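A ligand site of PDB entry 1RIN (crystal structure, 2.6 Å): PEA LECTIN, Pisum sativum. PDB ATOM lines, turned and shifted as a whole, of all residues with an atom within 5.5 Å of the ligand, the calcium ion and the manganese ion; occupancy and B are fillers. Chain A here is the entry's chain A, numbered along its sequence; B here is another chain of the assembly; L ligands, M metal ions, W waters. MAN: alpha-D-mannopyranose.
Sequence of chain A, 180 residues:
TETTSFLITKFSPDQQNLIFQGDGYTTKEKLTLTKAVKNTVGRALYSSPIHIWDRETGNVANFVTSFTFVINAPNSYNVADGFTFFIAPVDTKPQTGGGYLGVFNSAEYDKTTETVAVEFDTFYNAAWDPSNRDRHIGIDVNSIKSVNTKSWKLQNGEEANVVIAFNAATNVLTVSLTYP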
ATOM      1  N   ASN A  39      26.165 -26.833 -24.419  1.00  0.00           N
ATOM      2  CA  ASN A  39      26.792 -25.802 -23.597  1.00  0.00           C
ATOM      3  C   ASN A  39      27.422 -24.612 -24.331  1.00  0.00           C
ATOM      4  O   ASN A  39      28.607 -24.283 -24.228  1.00  0.00           O
ATOM      5  CB  ASN A  39      27.854 -26.460 -22.716  1.00  0.00           C
ATOM      6  CG  ASN A  39      27.347 -27.617 -21.878  1.00  0.00           C
ATOM      7  OD1 ASN A  39      26.523 -27.512 -20.984  1.00  0.00           O
ATOM      8  ND2 ASN A  39      27.803 -28.817 -22.142  1.00  0.00           N
ATOM      9  N   ALA A  80      16.446 -26.810 -25.061  1.00  0.00           N
ATOM     10  CA  ALA A  80      16.992 -25.895 -24.080  1.00  0.00           C
ATOM     11  C   ALA A  80      17.972 -24.916 -24.739  1.00  0.00           C
ATOM     12  O   ALA A  80      18.351 -25.120 -25.897  1.00  0.00           O
ATOM     13  CB  ALA A  80      17.724 -26.693 -23.026  1.00  0.00           C
ATOM     14  N   ASP A  81      18.374 -23.755 -24.220  1.00  0.00           N
ATOM     15  CA  ASP A  81      17.852 -23.164 -23.015  1.00  0.00           C
ATOM     16  C   ASP A  81      16.892 -22.018 -23.266  1.00  0.00           C
ATOM     17  O   ASP A  81      15.936 -21.772 -22.516  1.00  0.00           O
ATOM     18  CB  ASP A  81      18.947 -22.658 -22.228  1.00  0.00           C
ATOM     19  CG  ASP A  81      19.287 -23.773 -21.251  1.00  0.00           C
ATOM     20  OD1 ASP A  81      18.682 -23.895 -20.213  1.00  0.00           O
ATOM     21  OD2 ASP A  81      20.192 -24.576 -21.500  1.00  0.00           O
ATOM     22  N   GLY A  97      25.927 -19.100 -18.600  1.00  0.00           N
ATOM     23  CA  GLY A  97      25.269 -19.793 -19.682  1.00  0.00           C
ATOM     24  C   GLY A  97      24.165 -20.746 -19.249  1.00  0.00           C
ATOM     25  O   GLY A  97      23.531 -20.564 -18.184  1.00  0.00           O
ATOM     26  N   GLY A  98      23.909 -21.748 -20.080  1.00  0.00           N
ATOM     27  CA  GLY A  98      22.859 -22.717 -19.840  1.00  0.00           C
ATOM     28  C   GLY A  98      21.553 -22.087 -19.366  1.00  0.00           C
ATOM     29  O   GLY A  98      20.994 -21.184 -19.997  1.00  0.00           O
ATOM     30  N   GLY A  99      21.108 -22.412 -18.163  1.00  0.00           N
ATOM     31  CA  GLY A  99      19.835 -21.935 -17.672  1.00  0.00           C
ATOM     32  C   GLY A  99      19.784 -20.455 -17.411  1.00  0.00           C
ATOM     33  O   GLY A  99      18.704 -19.917 -17.249  1.00  0.00           O
ATOM     34  N   TYR A 100      20.927 -19.762 -17.345  1.00  0.00           N
ATOM     35  CA  TYR A 100      20.919 -18.307 -17.075  1.00  0.00           C
ATOM     36  C   TYR A 100      20.904 -17.423 -18.308  1.00  0.00           C
ATOM     37  O   TYR A 100      21.046 -16.196 -18.242  1.00  0.00           O
ATOM     38  CB  TYR A 100      22.111 -17.913 -16.233  1.00  0.00           C
ATOM     39  CG  TYR A 100      22.056 -18.543 -14.857  1.00  0.00           C
ATOM     40  CD1 TYR A 100      21.302 -17.961 -13.863  1.00  0.00           C
ATOM     41  CD2 TYR A 100      22.760 -19.687 -14.621  1.00  0.00           C
ATOM     42  CE1 TYR A 100      21.244 -18.525 -12.618  1.00  0.00           C
ATOM     43  CE2 TYR A 100      22.714 -20.257 -13.370  1.00  0.00           C
ATOM     44  CZ  TYR A 100      21.960 -19.675 -12.376  1.00  0.00           C
ATOM     45  OH  TYR A 100      21.903 -20.253 -11.131  1.00  0.00           O
ATOM     46  N   GLU A 119      12.622 -12.977 -21.633  1.00  0.00           N
ATOM     47  CA  GLU A 119      13.058 -14.310 -22.032  1.00  0.00           C
ATOM     48  C   GLU A 119      12.018 -15.150 -22.741  1.00  0.00           C
ATOM     49  O   GLU A 119      10.813 -14.961 -22.576  1.00  0.00           O
ATOM     50  CB  GLU A 119      13.524 -15.090 -20.849  1.00  0.00           C
ATOM     51  CG  GLU A 119      12.407 -15.324 -19.837  1.00  0.00           C
ATOM     52  CD  GLU A 119      12.764 -16.277 -18.726  1.00  0.00           C
ATOM     53  OE1 GLU A 119      13.760 -16.060 -18.078  1.00  0.00           O
ATOM     54  OE2 GLU A 119      12.032 -17.229 -18.523  1.00  0.00           O
ATOM     55  N   ASP A 121      11.910 -18.875 -22.718  1.00  0.00           N
ATOM     56  CA  ASP A 121      12.552 -19.983 -22.033  1.00  0.00           C
ATOM     57  C   ASP A 121      11.960 -21.339 -22.418  1.00  0.00           C
ATOM     58  O   ASP A 121      10.773 -21.638 -22.229  1.00  0.00           O
ATOM     59  CB  ASP A 121      12.417 -19.707 -20.540  1.00  0.00           C
ATOM     60  CG  ASP A 121      13.177 -20.584 -19.551  1.00  0.00           C
ATOM     61  OD1 ASP A 121      13.525 -21.717 -19.896  1.00  0.00           O
ATOM     62  OD2 ASP A 121      13.435 -20.147 -18.418  1.00  0.00           O
ATOM     63  N   THR A 122      12.831 -22.209 -22.945  1.00  0.00           N
ATOM     64  CA  THR A 122      12.413 -23.519 -23.435  1.00  0.00           C
ATOM     65  C   THR A 122      12.702 -24.704 -22.498  1.00  0.00           C
ATOM     66  O   THR A 122      12.261 -25.836 -22.691  1.00  0.00           O
ATOM     67  CB  THR A 122      13.057 -23.815 -24.775  1.00  0.00           C
ATOM     68  OG1 THR A 122      14.448 -23.673 -24.600  1.00  0.00           O
ATOM     69  CG2 THR A 122      12.623 -22.873 -25.868  1.00  0.00           C
ATOM     70  N   PHE A 123      13.374 -24.426 -21.379  1.00  0.00           N
ATOM     71  CA  PHE A 123      13.808 -25.466 -20.490  1.00  0.00           C
ATOM     72  C   PHE A 123      13.448 -25.168 -19.067  1.00  0.00           C
ATOM     73  O   PHE A 123      13.777 -24.098 -18.548  1.00  0.00           O
ATOM     74  CB  PHE A 123      15.320 -25.642 -20.554  1.00  0.00           C
ATOM     75  CG  PHE A 123      15.819 -26.887 -19.815  1.00  0.00           C
ATOM     76  CD1 PHE A 123      15.817 -28.112 -20.465  1.00  0.00           C
ATOM     77  CD2 PHE A 123      16.294 -26.762 -18.520  1.00  0.00           C
ATOM     78  CE1 PHE A 123      16.304 -29.233 -19.815  1.00  0.00           C
ATOM     79  CE2 PHE A 123      16.770 -27.869 -17.869  1.00  0.00           C
ATOM     80  CZ  PHE A 123      16.760 -29.102 -18.511  1.00  0.00           C
ATOM     81  N   TYR A 124      12.825 -26.154 -18.392  1.00  0.00           N
ATOM     82  CA  TYR A 124      12.418 -25.966 -17.008  1.00  0.00           C
ATOM     83  C   TYR A 124      13.606 -26.180 -16.083  1.00  0.00           C
ATOM     84  O   TYR A 124      14.244 -27.230 -16.049  1.00  0.00           O
ATOM     85  CB  TYR A 124      11.241 -26.956 -16.678  1.00  0.00           C
ATOM     86  CG  TYR A 124      10.829 -26.958 -15.207  1.00  0.00           C
ATOM     87  CD1 TYR A 124      10.162 -25.879 -14.638  1.00  0.00           C
ATOM     88  CD2 TYR A 124      11.210 -28.033 -14.423  1.00  0.00           C
ATOM     89  CE1 TYR A 124       9.897 -25.894 -13.280  1.00  0.00           C
ATOM     90  CE2 TYR A 124      10.946 -28.049 -13.065  1.00  0.00           C
ATOM     91  CZ  TYR A 124      10.295 -26.976 -12.519  1.00  0.00           C
ATOM     92  OH  TYR A 124      10.072 -27.002 -11.166  1.00  0.00           O
ATOM     93  N   ASN A 125      13.922 -25.161 -15.318  1.00  0.00           N
ATOM     94  CA  ASN A 125      14.941 -25.236 -14.297  1.00  0.00           C
ATOM     95  C   ASN A 125      14.231 -25.152 -12.960  1.00  0.00           C
ATOM     96  O   ASN A 125      13.727 -24.099 -12.534  1.00  0.00           O
ATOM     97  CB  ASN A 125      15.938 -24.075 -14.373  1.00  0.00           C
ATOM     98  CG  ASN A 125      16.748 -24.037 -15.657  1.00  0.00           C
ATOM     99  OD1 ASN A 125      16.418 -23.237 -16.516  1.00  0.00           O
ATOM    100  ND2 ASN A 125      17.799 -24.793 -15.921  1.00  0.00           N
ATOM    101  N   TRP A 128      13.934 -22.019 -10.182  1.00  0.00           N
ATOM    102  CA  TRP A 128      13.332 -20.681 -10.383  1.00  0.00           C
ATOM    103  C   TRP A 128      12.238 -20.649 -11.456  1.00  0.00           C
ATOM    104  O   TRP A 128      11.429 -19.733 -11.482  1.00  0.00           O
ATOM    105  CB  TRP A 128      14.415 -19.637 -10.780  1.00  0.00           C
ATOM    106  CG  TRP A 128      15.251 -19.999 -12.016  1.00  0.00           C
ATOM    107  CD1 TRP A 128      14.696 -19.902 -13.251  1.00  0.00           C
ATOM    108  CD2 TRP A 128      16.538 -20.519 -12.064  1.00  0.00           C
ATOM    109  NE1 TRP A 128      15.576 -20.369 -14.081  1.00  0.00           N
ATOM    110  CE2 TRP A 128      16.688 -20.753 -13.425  1.00  0.00           C
ATOM    111  CE3 TRP A 128      17.583 -20.852 -11.208  1.00  0.00           C
ATOM    112  CZ2 TRP A 128      17.861 -21.288 -13.935  1.00  0.00           C
ATOM    113  CZ3 TRP A 128      18.755 -21.387 -11.718  1.00  0.00           C
ATOM    114  CH2 TRP A 128      18.886 -21.601 -13.070  1.00  0.00           C
ATOM    115  N   ASP A 129      12.166 -21.653 -12.355  1.00  0.00           N
ATOM    116  CA  ASP A 129      11.157 -21.635 -13.403  1.00  0.00           C
ATOM    117  C   ASP A 129       9.752 -22.050 -12.958  1.00  0.00           C
ATOM    118  O   ASP A 129       9.628 -22.855 -12.023  1.00  0.00           O
ATOM    119  CB  ASP A 129      11.627 -22.513 -14.561  1.00  0.00           C
ATOM    120  CG  ASP A 129      12.597 -21.814 -15.507  1.00  0.00           C
ATOM    121  OD1 ASP A 129      12.606 -20.595 -15.601  1.00  0.00           O
ATOM    122  OD2 ASP A 129      13.349 -22.493 -16.204  1.00  0.00           O
ATOM    123  N   PRO A 130       8.674 -21.585 -13.615  1.00  0.00           N
ATOM    124  CA  PRO A 130       7.289 -21.895 -13.256  1.00  0.00           C
ATOM    125  C   PRO A 130       6.964 -23.353 -13.017  1.00  0.00           C
ATOM    126  O   PRO A 130       7.274 -24.254 -13.801  1.00  0.00           O
ATOM    127  CB  PRO A 130       6.446 -21.340 -14.363  1.00  0.00           C
ATOM    128  CG  PRO A 130       7.292 -20.301 -15.007  1.00  0.00           C
ATOM    129  CD  PRO A 130       8.676 -20.922 -14.921  1.00  0.00           C
ATOM    130  N   HIS A 136       7.822 -20.882 -21.584  1.00  0.00           N
ATOM    131  CA  HIS A 136       7.151 -19.654 -21.249  1.00  0.00           C
ATOM    132  C   HIS A 136       7.856 -18.407 -21.710  1.00  0.00           C
ATOM    133  O   HIS A 136       9.045 -18.388 -22.024  1.00  0.00           O
ATOM    134  CB  HIS A 136       6.950 -19.609 -19.695  1.00  0.00           C
ATOM    135  CG  HIS A 136       8.246 -19.769 -18.909  1.00  0.00           C
ATOM    136  ND1 HIS A 136       8.811 -20.938 -18.667  1.00  0.00           N
ATOM    137  CD2 HIS A 136       9.052 -18.762 -18.410  1.00  0.00           C
ATOM    138  CE1 HIS A 136       9.941 -20.719 -18.074  1.00  0.00           C
ATOM    139  NE2 HIS A 136      10.080 -19.405 -17.910  1.00  0.00           N
ATOM    140  N   ILE A 144      17.286 -14.286 -12.712  1.00  0.00           N
ATOM    141  CA  ILE A 144      16.797 -15.213 -13.728  1.00  0.00           C
ATOM    142  C   ILE A 144      15.400 -15.742 -13.351  1.00  0.00           C
ATOM    143  O   ILE A 144      14.702 -16.394 -14.122  1.00  0.00           O
ATOM    144  CB  ILE A 144      17.838 -16.343 -13.897  1.00  0.00           C
ATOM    145  CG1 ILE A 144      17.484 -17.174 -15.129  1.00  0.00           C
ATOM    146  CG2 ILE A 144      17.912 -17.216 -12.664  1.00  0.00           C
ATOM    147  CD1 ILE A 144      17.433 -16.401 -16.460  1.00  0.00           C
ATOM    148  N   SER A 146      11.961 -14.841 -13.217  1.00  0.00           N
ATOM    149  CA  SER A 146      11.099 -13.803 -13.770  1.00  0.00           C
ATOM    150  C   SER A 146      10.036 -13.177 -12.864  1.00  0.00           C
ATOM    151  O   SER A 146       9.321 -13.870 -12.116  1.00  0.00           O
ATOM    152  CB  SER A 146      10.318 -14.283 -14.972  1.00  0.00           C
ATOM    153  OG  SER A 146      10.958 -15.264 -15.763  1.00  0.00           O
ATOM    154  N   THR A 149       5.465 -14.411 -15.938  1.00  0.00           N
ATOM    155  CA  THR A 149       5.591 -15.364 -17.052  1.00  0.00           C
ATOM    156  C   THR A 149       4.259 -15.742 -17.726  1.00  0.00           C
ATOM    157  O   THR A 149       3.156 -15.486 -17.228  1.00  0.00           O
ATOM    158  CB  THR A 149       6.190 -16.711 -16.665  1.00  0.00           C
ATOM    159  OG1 THR A 149       5.252 -17.325 -15.798  1.00  0.00           O
ATOM    160  CG2 THR A 149       7.556 -16.600 -16.028  1.00  0.00           C
ATOM    161  N   THR B  28      22.632 -22.678 -24.846  1.00  0.00           N
ATOM    162  CA  THR B  28      22.361 -24.121 -24.715  1.00  0.00           C
ATOM    163  C   THR B  28      23.183 -24.668 -23.541  1.00  0.00           C
ATOM    164  O   THR B  28      24.146 -24.020 -23.121  1.00  0.00           O
ATOM    165  CB  THR B  28      22.756 -24.915 -25.930  1.00  0.00           C
ATOM    166  OG1 THR B  28      24.142 -24.791 -26.089  1.00  0.00           O
ATOM    167  CG2 THR B  28      22.096 -24.393 -27.189  1.00  0.00           C
ATOM    168  N   GLY B  29      22.807 -25.771 -22.902  1.00  0.00           N
ATOM    169  CA  GLY B  29      23.554 -26.325 -21.761  1.00  0.00           C
ATOM    170  C   GLY B  29      23.701 -27.810 -21.992  1.00  0.00           C
ATOM    171  O   GLY B  29      24.278 -28.207 -22.998  1.00  0.00           O
ATOM    172  N   ALA B  30      23.151 -28.687 -21.174  1.00  0.00           N
ATOM    173  CA  ALA B  30      23.210 -30.111 -21.496  1.00  0.00           C
ATOM    174  C   ALA B  30      22.329 -30.456 -22.690  1.00  0.00           C
ATOM    175  O   ALA B  30      22.519 -31.448 -23.369  1.00  0.00           O
ATOM    176  CB  ALA B  30      22.710 -30.968 -20.379  1.00  0.00           C
ATOM    177  N   GLU B  31      21.306 -29.641 -22.919  1.00  0.00           N
ATOM    178  CA  GLU B  31      20.434 -29.779 -24.087  1.00  0.00           C
ATOM    179  C   GLU B  31      20.462 -28.526 -24.970  1.00  0.00           C
ATOM    180  O   GLU B  31      20.962 -27.454 -24.596  1.00  0.00           O
ATOM    181  CB  GLU B  31      19.002 -30.012 -23.660  1.00  0.00           C
ATOM    182  CG  GLU B  31      18.892 -31.303 -22.878  1.00  0.00           C
ATOM    183  CD  GLU B  31      17.498 -31.733 -22.505  1.00  0.00           C
ATOM    184  OE1 GLU B  31      16.558 -30.947 -22.516  1.00  0.00           O
ATOM    185  OE2 GLU B  31      17.344 -32.913 -22.194  1.00  0.00           O
ATOM    186  N   TYR B  32      19.856 -28.616 -26.162  1.00  0.00           N
ATOM    187  CA  TYR B  32      20.086 -27.592 -27.163  1.00  0.00           C
ATOM    188  C   TYR B  32      19.103 -27.462 -28.334  1.00  0.00           C
ATOM    189  O   TYR B  32      18.189 -28.248 -28.548  1.00  0.00           O
ATOM    190  CB  TYR B  32      21.541 -27.828 -27.674  1.00  0.00           C
ATOM    191  CG  TYR B  32      21.747 -29.212 -28.225  1.00  0.00           C
ATOM    192  CD1 TYR B  32      21.304 -29.476 -29.504  1.00  0.00           C
ATOM    193  CD2 TYR B  32      22.311 -30.196 -27.462  1.00  0.00           C
ATOM    194  CE1 TYR B  32      21.404 -30.747 -30.037  1.00  0.00           C
ATOM    195  CE2 TYR B  32      22.412 -31.466 -27.982  1.00  0.00           C
ATOM    196  CZ  TYR B  32      21.967 -31.731 -29.274  1.00  0.00           C
ATOM    197  OH  TYR B  32      22.093 -32.994 -29.833  1.00  0.00           O
HETATM  198  C1  MAN L   1      22.173 -28.386 -17.581  1.00  0.00           C
HETATM  199  C2  MAN L   1      22.598 -26.977 -17.139  1.00  0.00           C
HETATM  200  C3  MAN L   1      21.373 -26.090 -17.036  1.00  0.00           C
HETATM  201  C4  MAN L   1      20.680 -26.069 -18.356  1.00  0.00           C
HETATM  202  C5  MAN L   1      20.342 -27.484 -18.767  1.00  0.00           C
HETATM  203  C6  MAN L   1      19.669 -27.527 -20.123  1.00  0.00           C
HETATM  204  O1  MAN L   1      21.344 -29.052 -16.619  1.00  0.00           O
HETATM  205  O2  MAN L   1      23.567 -26.425 -18.030  1.00  0.00           O
HETATM  206  O3  MAN L   1      21.691 -24.782 -16.611  1.00  0.00           O
HETATM  207  O4  MAN L   1      19.507 -25.327 -18.247  1.00  0.00           O
HETATM  208  O5  MAN L   1      21.522 -28.268 -18.847  1.00  0.00           O
HETATM  209  O6  MAN L   1      20.547 -27.292 -21.181  1.00  0.00           O
HETATM  210 CA    CA M   1      14.765 -22.146 -17.991  1.00  0.00          CA
HETATM  211 MN    MN M   2      12.222 -18.939 -17.115  1.00  0.00          MN
HETATM  212  O   HOH W   1      11.244 -17.887 -15.453  1.00  0.00           O
HETATM  213  O   HOH W   2      15.934 -20.374 -16.808  1.00  0.00           O
HETATM  214  O   HOH W   3      13.958 -18.067 -16.410  1.00  0.00           O
HETATM  215  O   HOH W   4      16.278 -22.600 -19.787  1.00  0.00           O
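N of Glu 31 of chain B lies within hydrogen-bond range of O6 of the ligand, 3.0 Å away.
OD1 of Asp 81 is in hydrogen-bond range of O4 of the ligand, 2.6 Å away.
An oxygen (O3) of the ligand is in hydrogen-bond range of the backbone NH of Gly 99, 2.9 Å away.
N of Ala 30 of chain B sits at hydrogen-bond distance from O5 of the ligand (2.9 Å).
O6 of the ligand sits close to N of Gly 29 of chain B (3.2 Å).
An oxygen (O6) of the ligand is in hydrogen-bond range of the backbone carbonyl oxygen of Glu 31 of chain B.
The side-chain amide nitrogen (ND2) of Asn 125 sits at hydrogen-bond distance from an oxygen (O4) of the ligand (2.9 Å).
The side-chain carboxylate of Asp 81 is in hydrogen-bond range of the backbone NH of Gly 29 of chain B, 3.2 Å away.
OD1 of Asp 129 lies close to NE1 of Trp 128.
O of Gly 29 of chain B sits at hydrogen-bond distance from N of Asn 39 (2.7 Å).
The backbone carbonyl oxygen (O) of Asp 81 sits at hydrogen-bond distance from the backbone NH (N) of Thr 122, at 3.2 Å.
Residues that only touch the ligand: Ala 80 and Gly 98.
Hydrophobic or aromatic side chains within 4 Å of the ligand: Ala 80, Phe 123 and Ala 30 of chain B.
Of the 25 residues printed, 9 come within 4 Å of the ligand.
Along chain A the residues within 4 Å of the ligand span positions 80 to 125.
Four residues have an atom within 4 Å of the calcium ion: Asp 121, Phe 123, Asn 125 and Asp 129.
The nearest printed residue that does not touch the calcium ion is Trp 128 (4.4 Å).
The calcium ion is bound by the backbone carbonyl oxygen (O) of Phe 123, the side-chain carboxylate (OD2) of Asp 129, the side-chain carboxylate (OD1) of Asp 121, water W4, water W2, the side-chain carboxylate (OD2) of Asp 121 and the side-chain amide oxygen (OD1) of Asn 125.
The manganese ion is bound by water W3 (2.1 Å), OD2 of Asp 121 (2.2 Å), water W1 (2.2 Å), OE2 of Glu 119 (2.2 Å), OD1 of Asp 129 (2.3 Å) and NE2 of His 136 (2.3 Å).
Water W2 lies within hydrogen-bond range of the indole nitrogen of Trp 128 (2.8 Å) and the backbone carbonyl oxygen of Gly 99 (2.8 Å).
Water W3 lies within hydrogen-bond range of the side-chain carboxylate (OE1) of Glu 119 and the backbone carbonyl oxygen (O) of Ile 144.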
